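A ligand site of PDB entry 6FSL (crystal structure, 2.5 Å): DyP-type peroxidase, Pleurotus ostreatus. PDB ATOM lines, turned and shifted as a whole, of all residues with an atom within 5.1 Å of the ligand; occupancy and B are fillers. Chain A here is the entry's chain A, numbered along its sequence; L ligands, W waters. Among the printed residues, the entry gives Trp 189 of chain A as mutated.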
ATOM      1  N   GLU A 185      14.024 -21.473  27.442  1.00  0.00           N
ATOM      2  CA  GLU A 185      14.634 -20.203  27.837  1.00  0.00           C
ATOM      3  C   GLU A 185      13.661 -19.028  27.572  1.00  0.00           C
ATOM      4  O   GLU A 185      12.591 -19.210  26.964  1.00  0.00           O
ATOM      5  CB  GLU A 185      16.030 -20.068  27.222  1.00  0.00           C
ATOM      6  CG  GLU A 185      16.124 -20.041  25.712  1.00  0.00           C
ATOM      7  CD  GLU A 185      15.531 -18.819  25.119  1.00  0.00           C
ATOM      8  OE1 GLU A 185      15.636 -17.758  25.739  1.00  0.00           O
ATOM      9  OE2 GLU A 185      14.948 -18.922  24.055  1.00  0.00           O
ATOM     10  N   PHE A 187      13.451 -16.239  25.732  1.00  0.00           N
ATOM     11  CA  PHE A 187      13.030 -15.872  24.366  1.00  0.00           C
ATOM     12  C   PHE A 187      11.961 -16.801  23.850  1.00  0.00           C
ATOM     13  O   PHE A 187      11.213 -16.389  22.961  1.00  0.00           O
ATOM     14  CB  PHE A 187      14.171 -15.863  23.345  1.00  0.00           C
ATOM     15  CG  PHE A 187      15.238 -14.864  23.611  1.00  0.00           C
ATOM     16  CD1 PHE A 187      14.925 -13.541  23.939  1.00  0.00           C
ATOM     17  CD2 PHE A 187      16.600 -15.217  23.494  1.00  0.00           C
ATOM     18  CE1 PHE A 187      15.926 -12.614  24.158  1.00  0.00           C
ATOM     19  CE2 PHE A 187      17.600 -14.290  23.713  1.00  0.00           C
ATOM     20  CZ  PHE A 187      17.252 -12.975  24.041  1.00  0.00           C
ATOM     21  N   TRP A 189      12.481 -20.541  23.384  1.00  0.00           N
ATOM     22  CA  TRP A 189      13.004 -21.763  22.753  1.00  0.00           C
ATOM     23  C   TRP A 189      13.285 -22.851  23.779  1.00  0.00           C
ATOM     24  O   TRP A 189      13.868 -22.563  24.835  1.00  0.00           O
ATOM     25  CB  TRP A 189      14.297 -21.453  21.978  1.00  0.00           C
ATOM     26  CG  TRP A 189      14.046 -20.999  20.606  1.00  0.00           C
ATOM     27  CD1 TRP A 189      14.188 -21.728  19.445  1.00  0.00           C
ATOM     28  CD2 TRP A 189      13.572 -19.716  20.222  1.00  0.00           C
ATOM     29  NE1 TRP A 189      13.837 -20.959  18.366  1.00  0.00           N
ATOM     30  CE2 TRP A 189      13.449 -19.723  18.808  1.00  0.00           C
ATOM     31  CE3 TRP A 189      13.228 -18.564  20.928  1.00  0.00           C
ATOM     32  CZ2 TRP A 189      12.986 -18.627  18.090  1.00  0.00           C
ATOM     33  CZ3 TRP A 189      12.769 -17.447  20.216  1.00  0.00           C
ATOM     34  CH2 TRP A 189      12.649 -17.495  18.808  1.00  0.00           C
ATOM     35  N   LEU A 190      12.905 -24.087  23.452  1.00  0.00           N
ATOM     36  CA  LEU A 190      13.281 -25.277  24.215  1.00  0.00           C
ATOM     37  C   LEU A 190      14.783 -25.400  24.284  1.00  0.00           C
ATOM     38  O   LEU A 190      15.435 -25.464  23.251  1.00  0.00           O
ATOM     39  CB  LEU A 190      12.734 -26.553  23.545  1.00  0.00           C
ATOM     40  CG  LEU A 190      12.956 -27.895  24.250  1.00  0.00           C
ATOM     41  CD1 LEU A 190      12.443 -27.873  25.686  1.00  0.00           C
ATOM     42  CD2 LEU A 190      12.256 -29.000  23.460  1.00  0.00           C
ATOM     43  N   ASP A 191      15.322 -25.430  25.484  1.00  0.00           N
ATOM     44  CA  ASP A 191      16.756 -25.433  25.681  1.00  0.00           C
ATOM     45  C   ASP A 191      17.130 -26.708  26.341  1.00  0.00           C
ATOM     46  O   ASP A 191      16.314 -27.307  27.018  1.00  0.00           O
ATOM     47  CB  ASP A 191      17.205 -24.268  26.578  1.00  0.00           C
ATOM     48  CG  ASP A 191      18.675 -23.905  26.395  1.00  0.00           C
ATOM     49  OD1 ASP A 191      19.302 -24.390  25.412  1.00  0.00           O
ATOM     50  OD2 ASP A 191      19.208 -23.116  27.204  1.00  0.00           O
ATOM     51  N   GLY A 192      18.389 -27.110  26.172  1.00  0.00           N
ATOM     52  CA  GLY A 192      18.910 -28.328  26.780  1.00  0.00           C
ATOM     53  C   GLY A 192      18.828 -29.581  25.917  1.00  0.00           C
ATOM     54  O   GLY A 192      18.967 -30.700  26.436  1.00  0.00           O
ATOM     55  N   ILE A 193      18.612 -29.401  24.616  1.00  0.00           N
ATOM     56  CA  ILE A 193      18.441 -30.514  23.690  1.00  0.00           C
ATOM     57  C   ILE A 193      19.753 -31.194  23.290  1.00  0.00           C
ATOM     58  O   ILE A 193      19.885 -32.396  23.404  1.00  0.00           O
ATOM     59  CB  ILE A 193      17.665 -30.071  22.453  1.00  0.00           C
ATOM     60  CG1 ILE A 193      16.280 -29.562  22.877  1.00  0.00           C
ATOM     61  CG2 ILE A 193      17.509 -31.228  21.479  1.00  0.00           C
ATOM     62  CD1 ILE A 193      15.507 -28.892  21.763  1.00  0.00           C
ATOM     63  N   SER A 194      20.739 -30.432  22.828  1.00  0.00           N
ATOM     64  CA  SER A 194      21.942 -31.032  22.281  1.00  0.00           C
ATOM     65  C   SER A 194      23.121 -30.905  23.246  1.00  0.00           C
ATOM     66  O   SER A 194      23.632 -29.826  23.453  1.00  0.00           O
ATOM     67  CB  SER A 194      22.243 -30.387  20.926  1.00  0.00           C
ATOM     68  OG  SER A 194      23.232 -31.112  20.205  1.00  0.00           O
ATOM     69  N   LEU A 245      23.907 -13.968  32.054  1.00  0.00           N
ATOM     70  CA  LEU A 245      23.437 -13.405  30.784  1.00  0.00           C
ATOM     71  C   LEU A 245      22.010 -12.932  30.897  1.00  0.00           C
ATOM     72  O   LEU A 245      21.098 -13.725  31.039  1.00  0.00           O
ATOM     73  CB  LEU A 245      23.565 -14.448  29.665  1.00  0.00           C
ATOM     74  CG  LEU A 245      24.950 -15.053  29.412  1.00  0.00           C
ATOM     75  CD1 LEU A 245      24.901 -16.094  28.303  1.00  0.00           C
ATOM     76  CD2 LEU A 245      25.957 -13.968  29.092  1.00  0.00           C
ATOM     77  N   GLN A 247      18.631 -11.303  29.364  1.00  0.00           N
ATOM     78  CA  GLN A 247      17.941 -11.361  28.085  1.00  0.00           C
ATOM     79  C   GLN A 247      16.956 -10.221  27.973  1.00  0.00           C
ATOM     80  O   GLN A 247      16.260  -9.913  28.922  1.00  0.00           O
ATOM     81  CB  GLN A 247      17.227 -12.694  27.935  1.00  0.00           C
ATOM     82  CG  GLN A 247      18.209 -13.837  27.816  1.00  0.00           C
ATOM     83  CD  GLN A 247      17.575 -15.201  27.626  1.00  0.00           C
ATOM     84  OE1 GLN A 247      16.984 -15.462  26.594  1.00  0.00           O
ATOM     85  NE2 GLN A 247      17.739 -16.062  28.590  1.00  0.00           N
ATOM     86  N   VAL A 280      18.043 -19.029  15.321  1.00  0.00           N
ATOM     87  CA  VAL A 280      18.414 -20.007  16.367  1.00  0.00           C
ATOM     88  C   VAL A 280      18.899 -21.329  15.727  1.00  0.00           C
ATOM     89  O   VAL A 280      19.844 -21.923  16.220  1.00  0.00           O
ATOM     90  CB  VAL A 280      17.240 -20.216  17.359  1.00  0.00           C
ATOM     91  CG1 VAL A 280      17.590 -21.269  18.400  1.00  0.00           C
ATOM     92  CG2 VAL A 280      16.902 -18.907  18.053  1.00  0.00           C
ATOM     93  N   ARG A 282      16.441 -23.734  15.289  1.00  0.00           N
ATOM     94  CA  ARG A 282      15.317 -24.565  15.721  1.00  0.00           C
ATOM     95  C   ARG A 282      14.074 -23.737  15.872  1.00  0.00           C
ATOM     96  O   ARG A 282      14.187 -22.546  16.176  1.00  0.00           O
ATOM     97  CB  ARG A 282      15.581 -25.190  17.077  1.00  0.00           C
ATOM     98  CG  ARG A 282      16.593 -26.297  17.105  1.00  0.00           C
ATOM     99  CD  ARG A 282      16.787 -26.779  18.531  1.00  0.00           C
ATOM    100  NE  ARG A 282      17.934 -27.684  18.579  1.00  0.00           N
ATOM    101  CZ  ARG A 282      17.915 -28.979  18.288  1.00  0.00           C
ATOM    102  NH1 ARG A 282      16.803 -29.581  17.936  1.00  0.00           N
ATOM    103  NH2 ARG A 282      19.033 -29.689  18.385  1.00  0.00           N
ATOM    104  N   ASN A 308      17.533 -34.439  17.012  1.00  0.00           N
ATOM    105  CA  ASN A 308      18.924 -34.037  16.885  1.00  0.00           C
ATOM    106  C   ASN A 308      19.716 -34.776  15.807  1.00  0.00           C
ATOM    107  O   ASN A 308      20.934 -34.611  15.759  1.00  0.00           O
ATOM    108  CB  ASN A 308      19.631 -34.136  18.249  1.00  0.00           C
ATOM    109  CG  ASN A 308      20.678 -33.081  18.405  1.00  0.00           C
ATOM    110  OD1 ASN A 308      20.541 -31.999  17.854  1.00  0.00           O
ATOM    111  ND2 ASN A 308      21.721 -33.366  19.147  1.00  0.00           N
ATOM    112  N   HIS A 329      22.385 -19.818  15.480  1.00  0.00           N
ATOM    113  CA  HIS A 329      23.066 -19.968  16.768  1.00  0.00           C
ATOM    114  C   HIS A 329      23.688 -21.345  16.936  1.00  0.00           C
ATOM    115  O   HIS A 329      24.908 -21.470  17.175  1.00  0.00           O
ATOM    116  CB  HIS A 329      22.093 -19.675  17.936  1.00  0.00           C
ATOM    117  CG  HIS A 329      22.660 -19.938  19.296  1.00  0.00           C
ATOM    118  ND1 HIS A 329      23.820 -19.364  19.744  1.00  0.00           N
ATOM    119  CD2 HIS A 329      22.214 -20.710  20.315  1.00  0.00           C
ATOM    120  CE1 HIS A 329      24.065 -19.757  20.981  1.00  0.00           C
ATOM    121  NE2 HIS A 329      23.101 -20.570  21.351  1.00  0.00           N
ATOM    122  N   ILE A 330      22.875 -22.390  16.774  1.00  0.00           N
ATOM    123  CA  ILE A 330      23.349 -23.764  17.017  1.00  0.00           C
ATOM    124  C   ILE A 330      24.474 -24.192  16.037  1.00  0.00           C
ATOM    125  O   ILE A 330      25.299 -25.066  16.358  1.00  0.00           O
ATOM    126  CB  ILE A 330      22.208 -24.814  17.056  1.00  0.00           C
ATOM    127  CG1 ILE A 330      21.569 -25.079  15.680  1.00  0.00           C
ATOM    128  CG2 ILE A 330      21.144 -24.457  18.071  1.00  0.00           C
ATOM    129  CD1 ILE A 330      20.812 -26.386  15.605  1.00  0.00           C
ATOM    130  N   THR A 333      27.784 -22.460  17.181  1.00  0.00           N
ATOM    131  CA  THR A 333      28.380 -23.062  18.379  1.00  0.00           C
ATOM    132  C   THR A 333      28.700 -24.556  18.283  1.00  0.00           C
ATOM    133  O   THR A 333      29.484 -25.021  19.039  1.00  0.00           O
ATOM    134  CB  THR A 333      27.448 -22.865  19.564  1.00  0.00           C
ATOM    135  OG1 THR A 333      26.182 -23.484  19.267  1.00  0.00           O
ATOM    136  CG2 THR A 333      27.252 -21.378  19.821  1.00  0.00           C
ATOM    137  N   TYR A 334      28.039 -25.306  17.402  1.00  0.00           N
ATOM    138  CA  TYR A 334      28.456 -26.674  17.022  1.00  0.00           C
ATOM    139  C   TYR A 334      28.249 -26.845  15.519  1.00  0.00           C
ATOM    140  O   TYR A 334      27.109 -27.115  15.040  1.00  0.00           O
ATOM    141  CB  TYR A 334      27.719 -27.739  17.841  1.00  0.00           C
ATOM    142  CG  TYR A 334      28.040 -29.181  17.493  1.00  0.00           C
ATOM    143  CD1 TYR A 334      29.329 -29.596  17.172  1.00  0.00           C
ATOM    144  CD2 TYR A 334      27.033 -30.164  17.569  1.00  0.00           C
ATOM    145  CE1 TYR A 334      29.608 -30.929  16.880  1.00  0.00           C
ATOM    146  CE2 TYR A 334      27.296 -31.502  17.302  1.00  0.00           C
ATOM    147  CZ  TYR A 334      28.586 -31.884  16.954  1.00  0.00           C
ATOM    148  OH  TYR A 334      28.836 -33.213  16.668  1.00  0.00           O
ATOM    149  N   ARG A 336      29.037 -29.104  13.401  1.00  0.00           N
ATOM    150  CA  ARG A 336      28.740 -30.406  12.836  1.00  0.00           C
ATOM    151  C   ARG A 336      29.534 -30.580  11.508  1.00  0.00           C
ATOM    152  O   ARG A 336      30.744 -30.349  11.493  1.00  0.00           O
ATOM    153  CB  ARG A 336      27.212 -30.584  12.733  1.00  0.00           C
ATOM    154  CG  ARG A 336      26.499 -30.402  14.065  1.00  0.00           C
ATOM    155  CD  ARG A 336      25.045 -30.803  13.997  1.00  0.00           C
ATOM    156  NE  ARG A 336      24.279 -30.365  15.183  1.00  0.00           N
ATOM    157  CZ  ARG A 336      23.348 -31.090  15.845  1.00  0.00           C
ATOM    158  NH1 ARG A 336      23.020 -32.320  15.456  1.00  0.00           N
ATOM    159  NH2 ARG A 336      22.725 -30.592  16.929  1.00  0.00           N
ATOM    160  N   ARG A 352      33.634 -28.995  21.973  1.00  0.00           N
ATOM    161  CA  ARG A 352      32.351 -29.350  22.564  1.00  0.00           C
ATOM    162  C   ARG A 352      32.266 -28.908  24.001  1.00  0.00           C
ATOM    163  O   ARG A 352      33.275 -28.804  24.662  1.00  0.00           O
ATOM    164  CB  ARG A 352      32.110 -30.861  22.458  1.00  0.00           C
ATOM    165  CG  ARG A 352      32.244 -31.428  21.050  1.00  0.00           C
ATOM    166  CD  ARG A 352      31.338 -30.754  20.044  1.00  0.00           C
ATOM    167  NE  ARG A 352      29.945 -30.739  20.454  1.00  0.00           N
ATOM    168  CZ  ARG A 352      29.127 -31.796  20.430  1.00  0.00           C
ATOM    169  NH1 ARG A 352      29.559 -33.013  20.007  1.00  0.00           N
ATOM    170  NH2 ARG A 352      27.855 -31.628  20.804  1.00  0.00           N
ATOM    171  N   ILE A 353      31.038 -28.592  24.435  1.00  0.00           N
ATOM    172  CA  ILE A 353      30.771 -28.227  25.837  1.00  0.00           C
ATOM    173  C   ILE A 353      29.474 -28.873  26.320  1.00  0.00           C
ATOM    174  O   ILE A 353      28.543 -29.084  25.529  1.00  0.00           O
ATOM    175  CB  ILE A 353      30.704 -26.708  26.038  1.00  0.00           C
ATOM    176  CG1 ILE A 353      29.833 -26.042  24.981  1.00  0.00           C
ATOM    177  CG2 ILE A 353      32.095 -26.094  25.968  1.00  0.00           C
ATOM    178  CD1 ILE A 353      29.450 -24.605  25.350  1.00  0.00           C
ATOM    179  N   ARG A 355      26.366 -28.139  28.650  1.00  0.00           N
ATOM    180  CA  ARG A 355      25.649 -27.004  29.211  1.00  0.00           C
ATOM    181  C   ARG A 355      24.726 -27.456  30.322  1.00  0.00           C
ATOM    182  O   ARG A 355      24.073 -28.492  30.227  1.00  0.00           O
ATOM    183  CB  ARG A 355      24.860 -26.299  28.131  1.00  0.00           C
ATOM    184  CG  ARG A 355      25.773 -25.721  27.077  1.00  0.00           C
ATOM    185  CD  ARG A 355      24.972 -25.106  25.945  1.00  0.00           C
ATOM    186  NE  ARG A 355      24.266 -26.144  25.202  1.00  0.00           N
ATOM    187  CZ  ARG A 355      22.959 -26.191  24.955  1.00  0.00           C
ATOM    188  NH1 ARG A 355      22.124 -25.240  25.318  1.00  0.00           N
ATOM    189  NH2 ARG A 355      22.484 -27.224  24.264  1.00  0.00           N
ATOM    190  N   LEU A 380      19.454 -15.980  31.581  1.00  0.00           N
ATOM    191  CA  LEU A 380      19.990 -17.318  31.668  1.00  0.00           C
ATOM    192  C   LEU A 380      21.246 -17.257  32.499  1.00  0.00           C
ATOM    193  O   LEU A 380      22.145 -16.473  32.178  1.00  0.00           O
ATOM    194  CB  LEU A 380      20.307 -17.848  30.287  1.00  0.00           C
ATOM    195  CG  LEU A 380      20.787 -19.306  30.179  1.00  0.00           C
ATOM    196  CD1 LEU A 380      19.618 -20.273  30.385  1.00  0.00           C
ATOM    197  CD2 LEU A 380      21.456 -19.546  28.818  1.00  0.00           C
ATOM    198  N   PHE A 382      24.133 -19.101  32.568  1.00  0.00           N
ATOM    199  CA  PHE A 382      24.828 -20.008  31.658  1.00  0.00           C
ATOM    200  C   PHE A 382      26.009 -20.639  32.352  1.00  0.00           C
ATOM    201  O   PHE A 382      26.851 -19.947  32.902  1.00  0.00           O
ATOM    202  CB  PHE A 382      25.305 -19.264  30.436  1.00  0.00           C
ATOM    203  CG  PHE A 382      26.091 -20.096  29.479  1.00  0.00           C
ATOM    204  CD1 PHE A 382      27.432 -20.295  29.682  1.00  0.00           C
ATOM    205  CD2 PHE A 382      25.502 -20.616  28.344  1.00  0.00           C
ATOM    206  CE1 PHE A 382      28.164 -21.042  28.805  1.00  0.00           C
ATOM    207  CE2 PHE A 382      26.237 -21.392  27.451  1.00  0.00           C
ATOM    208  CZ  PHE A 382      27.580 -21.603  27.690  1.00  0.00           C
ATOM    209  N   PHE A 393      34.567 -22.877  25.387  1.00  0.00           N
ATOM    210  CA  PHE A 393      33.765 -21.684  25.498  1.00  0.00           C
ATOM    211  C   PHE A 393      34.419 -20.427  24.884  1.00  0.00           C
ATOM    212  O   PHE A 393      33.793 -19.750  24.093  1.00  0.00           O
ATOM    213  CB  PHE A 393      33.431 -21.390  26.962  1.00  0.00           C
ATOM    214  CG  PHE A 393      32.884 -20.027  27.175  1.00  0.00           C
ATOM    215  CD1 PHE A 393      31.549 -19.771  26.914  1.00  0.00           C
ATOM    216  CD2 PHE A 393      33.690 -18.982  27.585  1.00  0.00           C
ATOM    217  CE1 PHE A 393      31.012 -18.506  27.101  1.00  0.00           C
ATOM    218  CE2 PHE A 393      33.182 -17.721  27.765  1.00  0.00           C
ATOM    219  CZ  PHE A 393      31.838 -17.479  27.520  1.00  0.00           C
ATOM    220  N   ILE A 396      34.683 -20.711  21.032  1.00  0.00           N
ATOM    221  CA  ILE A 396      33.325 -20.662  20.473  1.00  0.00           C
ATOM    222  C   ILE A 396      32.855 -19.221  20.426  1.00  0.00           C
ATOM    223  O   ILE A 396      32.345 -18.768  19.407  1.00  0.00           O
ATOM    224  CB  ILE A 396      32.302 -21.482  21.297  1.00  0.00           C
ATOM    225  CG1 ILE A 396      32.651 -22.977  21.303  1.00  0.00           C
ATOM    226  CG2 ILE A 396      30.902 -21.316  20.700  1.00  0.00           C
ATOM    227  CD1 ILE A 396      31.862 -23.812  22.307  1.00  0.00           C
ATOM    228  N   GLN A 397      33.020 -18.524  21.535  1.00  0.00           N
ATOM    229  CA  GLN A 397      32.598 -17.123  21.607  1.00  0.00           C
ATOM    230  C   GLN A 397      33.419 -16.211  20.627  1.00  0.00           C
ATOM    231  O   GLN A 397      32.832 -15.409  19.911  1.00  0.00           O
ATOM    232  CB  GLN A 397      32.633 -16.617  23.085  1.00  0.00           C
ATOM    233  CG  GLN A 397      32.070 -15.219  23.332  1.00  0.00           C
ATOM    234  CD  GLN A 397      30.551 -15.125  23.185  1.00  0.00           C
ATOM    235  OE1 GLN A 397      29.810 -15.743  23.918  1.00  0.00           O
ATOM    236  NE2 GLN A 397      30.097 -14.288  22.261  1.00  0.00           N
ATOM    237  N   ILE A 430      22.246 -14.200  18.660  1.00  0.00           N
ATOM    238  CA  ILE A 430      21.833 -14.449  20.030  1.00  0.00           C
ATOM    239  C   ILE A 430      22.938 -14.018  20.978  1.00  0.00           C
ATOM    240  O   ILE A 430      22.710 -13.149  21.815  1.00  0.00           O
ATOM    241  CB  ILE A 430      21.431 -15.944  20.198  1.00  0.00           C
ATOM    242  CG1 ILE A 430      20.226 -16.268  19.318  1.00  0.00           C
ATOM    243  CG2 ILE A 430      21.081 -16.299  21.644  1.00  0.00           C
ATOM    244  CD1 ILE A 430      18.989 -15.437  19.569  1.00  0.00           C
ATOM    245  N   ILE A 431      24.142 -14.576  20.801  1.00  0.00           N
ATOM    246  CA  ILE A 431      25.295 -14.333  21.667  1.00  0.00           C
ATOM    247  C   ILE A 431      26.507 -13.583  21.068  1.00  0.00           C
ATOM    248  O   ILE A 431      27.475 -13.268  21.796  1.00  0.00           O
ATOM    249  CB  ILE A 431      25.866 -15.666  22.174  1.00  0.00           C
ATOM    250  CG1 ILE A 431      26.279 -16.594  21.019  1.00  0.00           C
ATOM    251  CG2 ILE A 431      24.874 -16.350  23.046  1.00  0.00           C
ATOM    252  CD1 ILE A 431      27.324 -17.601  21.427  1.00  0.00           C
ATOM    253  N   VAL A 462      21.085 -10.122  24.255  1.00  0.00           N
ATOM    254  CA  VAL A 462      21.735 -10.750  25.397  1.00  0.00           C
ATOM    255  C   VAL A 462      22.869  -9.857  25.898  1.00  0.00           C
ATOM    256  O   VAL A 462      23.693  -9.412  25.119  1.00  0.00           O
ATOM    257  CB  VAL A 462      22.296 -12.128  25.021  1.00  0.00           C
ATOM    258  CG1 VAL A 462      23.093 -12.766  26.182  1.00  0.00           C
ATOM    259  CG2 VAL A 462      21.158 -13.013  24.543  1.00  0.00           C
HETATM  260  C1  LIG L   1      22.200 -24.541  21.872  1.00  0.00           C
HETATM  261  C2  LIG L   1      19.892 -20.614  23.389  1.00  0.00           C
HETATM  262  C3  LIG L   1      24.062 -18.785  25.146  1.00  0.00           C
HETATM  263  C4  LIG L   1      26.383 -22.492  23.084  1.00  0.00           C
HETATM  264  C5  LIG L   1      21.200 -23.641  22.168  1.00  0.00           C
HETATM  265  C6  LIG L   1      19.816 -23.821  21.831  1.00  0.00           C
HETATM  266  C7  LIG L   1      19.192 -22.696  22.256  1.00  0.00           C
HETATM  267  C8  LIG L   1      20.170 -21.833  22.833  1.00  0.00           C
HETATM  268  C9  LIG L   1      17.691 -22.387  22.156  1.00  0.00           C
HETATM  269  C10 LIG L   1      19.146 -24.955  21.114  1.00  0.00           C
HETATM  270  C11 LIG L   1      18.540 -26.040  22.012  1.00  0.00           C
HETATM  271  C12 LIG L   1      19.631 -26.904  22.552  1.00  0.00           C
HETATM  272  O1  LIG L   1      20.293 -27.615  21.807  1.00  0.00           O
HETATM  273  O2  LIG L   1      19.885 -26.904  23.771  1.00  0.00           O
HETATM  274  C13 LIG L   1      20.827 -19.786  24.039  1.00  0.00           C
HETATM  275  C14 LIG L   1      20.467 -18.584  24.720  1.00  0.00           C
HETATM  276  C15 LIG L   1      21.619 -18.047  25.227  1.00  0.00           C
HETATM  277  C16 LIG L   1      22.712 -18.990  24.838  1.00  0.00           C
HETATM  278  C17 LIG L   1      19.087 -18.009  24.849  1.00  0.00           C
HETATM  279  C18 LIG L   1      21.842 -16.799  26.023  1.00  0.00           C
HETATM  280  C19 LIG L   1      20.918 -15.943  26.417  1.00  0.00           C
HETATM  281  C20 LIG L   1      25.102 -19.625  24.721  1.00  0.00           C
HETATM  282  C21 LIG L   1      26.484 -19.437  24.950  1.00  0.00           C
HETATM  283  C22 LIG L   1      27.144 -20.519  24.352  1.00  0.00           C
HETATM  284  C23 LIG L   1      26.149 -21.333  23.752  1.00  0.00           C
HETATM  285  C24 LIG L   1      27.105 -18.296  25.721  1.00  0.00           C
HETATM  286  C25 LIG L   1      28.602 -20.768  24.210  1.00  0.00           C
HETATM  287  C26 LIG L   1      29.531 -19.812  24.258  1.00  0.00           C
HETATM  288  C27 LIG L   1      25.400 -23.346  22.639  1.00  0.00           C
HETATM  289  C28 LIG L   1      25.761 -24.682  22.098  1.00  0.00           C
HETATM  290  C29 LIG L   1      24.584 -25.229  21.776  1.00  0.00           C
HETATM  291  C30 LIG L   1      23.533 -24.262  22.114  1.00  0.00           C
HETATM  292  C31 LIG L   1      27.143 -25.356  21.936  1.00  0.00           C
HETATM  293  C32 LIG L   1      24.437 -26.580  21.200  1.00  0.00           C
HETATM  294  C33 LIG L   1      24.680 -26.635  19.705  1.00  0.00           C
HETATM  295  C34 LIG L   1      24.270 -28.030  19.241  1.00  0.00           C
HETATM  296  O3  LIG L   1      23.337 -28.124  18.390  1.00  0.00           O
HETATM  297  O4  LIG L   1      24.857 -29.042  19.755  1.00  0.00           O
HETATM  298  N1  LIG L   1      21.389 -22.380  22.704  1.00  0.00           N
HETATM  299  N2  LIG L   1      22.155 -19.944  24.087  1.00  0.00           N
HETATM  300  N3  LIG L   1      24.932 -20.739  23.940  1.00  0.00           N
HETATM  301  N4  LIG L   1      24.071 -23.116  22.593  1.00  0.00           N
HETATM  302 FE1  LIG L   1      23.150 -21.616  23.297  1.00  0.00          FE
HETATM  303  O   HOH W   1      26.524 -29.564  21.947  1.00  0.00           O
HETATM  304  O   HOH W   2      24.065 -27.490  15.619  1.00  0.00           O
HETATM  305  O   HOH W   3      20.917 -27.862  19.117  1.00  0.00           O
HETATM  306  O   HOH W   4      22.195 -22.372  26.475  1.00  0.00           O
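An iron atom (FE1) of the ligand is bound by a ring nitrogen (NE2) of His 329, at 2.2 Å.
An oxygen (O2) of the ligand lies within salt-bridge range of the guanidinium group of Arg 355 (2.7 Å).
O1 of the ligand is in hydrogen-bond range of N of Ser 194 (3.0 Å).
OG of Ser 194 lies within hydrogen-bond range of O4 of the ligand (2.7 Å).
An oxygen (O2) of the ligand is in hydrogen-bond range of the backbone NH (N) of Gly 192.
O2 of the ligand is in hydrogen-bond range of N of Ile 193 (2.9 Å).
The guanidinium group (NH2) of Arg 336 lies within salt-bridge range of an oxygen (O3) of the ligand (2.9 Å).
The side-chain carboxylate (OD1) of Asp 191 lies close to an oxygen (O2) of the ligand (3.1 Å).
NE of Arg 282 is in salt-bridge range of O1 of the ligand (3.999 Å).
OE1 of Glu 185 touches C17 of the ligand (3.6 Å).
CD2 of Phe 187 touches C17 of the ligand (3.98 Å).
Trp 189 touches the ligand (CB to C9, 3.5 Å).
Leu 190 touches the ligand (O to C11, 3.4 Å).
Leu 245 touches the ligand.
CD of Gln 247 touches C19 of the ligand, at 3.6 Å.
CG1 of Val 280 touches C9 of the ligand, 3.9 Å away.
Ile 330 touches the ligand (CG2 to C10, 3.7 Å).
Thr 333 touches the ligand (OG1 to C28, 3.1 Å).
Tyr 334 touches the ligand.
CD2 of Leu 380 touches C15 of the ligand (3.9 Å).
Phe 382 touches the ligand.
Phe 393 touches the ligand (CD1 to C26, 3.3 Å).
Ile 430 touches the ligand.
Ile 431 touches the ligand.
CG2 of Val 462 touches C19 of the ligand, at 3.5 Å.
Hydrophobic or aromatic side chains that line the ligand: Phe 187, Trp 189, Ile 193, Leu 245, Val 280, His 329, Ile 330, Tyr 334, Leu 380, Phe 382, Phe 393, Ile 430, Ile 431 and Val 462.
Of the 29 residues printed, 24 come within 4 Å of the ligand.
The nearest printed residue that does not touch the ligand is Ile 353 (4.1 Å).
Water W3 lies within hydrogen-bond range of O3 of the ligand (2.5 Å) and NH2 of Arg 282 (2.7 Å).
Water W1 lies within hydrogen-bond range of NH2 of Arg 352 (2.7 Å), O4 of the ligand (2.8 Å) and O of Ser 194 (3.3 Å).
Water W2 lies within hydrogen-bond range of O of Ile 330, NE of Arg 336, O3 of the ligand and O of Tyr 334.
Water W4 lies within hydrogen-bond range of NH1 of Arg 355 (3.1 Å) and OD2 of Asp 191 (3.2 Å).
OD1 of Asp 191 lies within salt-bridge range of NH1 of Arg 355, at 2.9 Å.
The side-chain hydroxyl (OG) of Ser 194 sits at hydrogen-bond distance from the guanidinium group (NH2) of Arg 336 (3.4 Å).
The side-chain amide oxygen (OD1) of Asn 308 lies within hydrogen-bond range of the guanidinium group (NH2) of Arg 336 (2.8 Å).
The side-chain hydroxyl of Tyr 334 lies close to the guanidinium group of Arg 352 (3.4 Å).
O of Ile 431 lies within hydrogen-bond range of NE2 of Gln 397 (2.9 Å).
N of Trp 189 is in hydrogen-bond range of OE2 of Glu 185 (3.0 Å).
The backbone NH (N) of Phe 187 sits at hydrogen-bond distance from the side-chain carboxylate (OE1) of Glu 185, 2.7 Å away.
OD1 of Asn 308 sits at hydrogen-bond distance from NH2 of Arg 282, 2.8 Å away.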
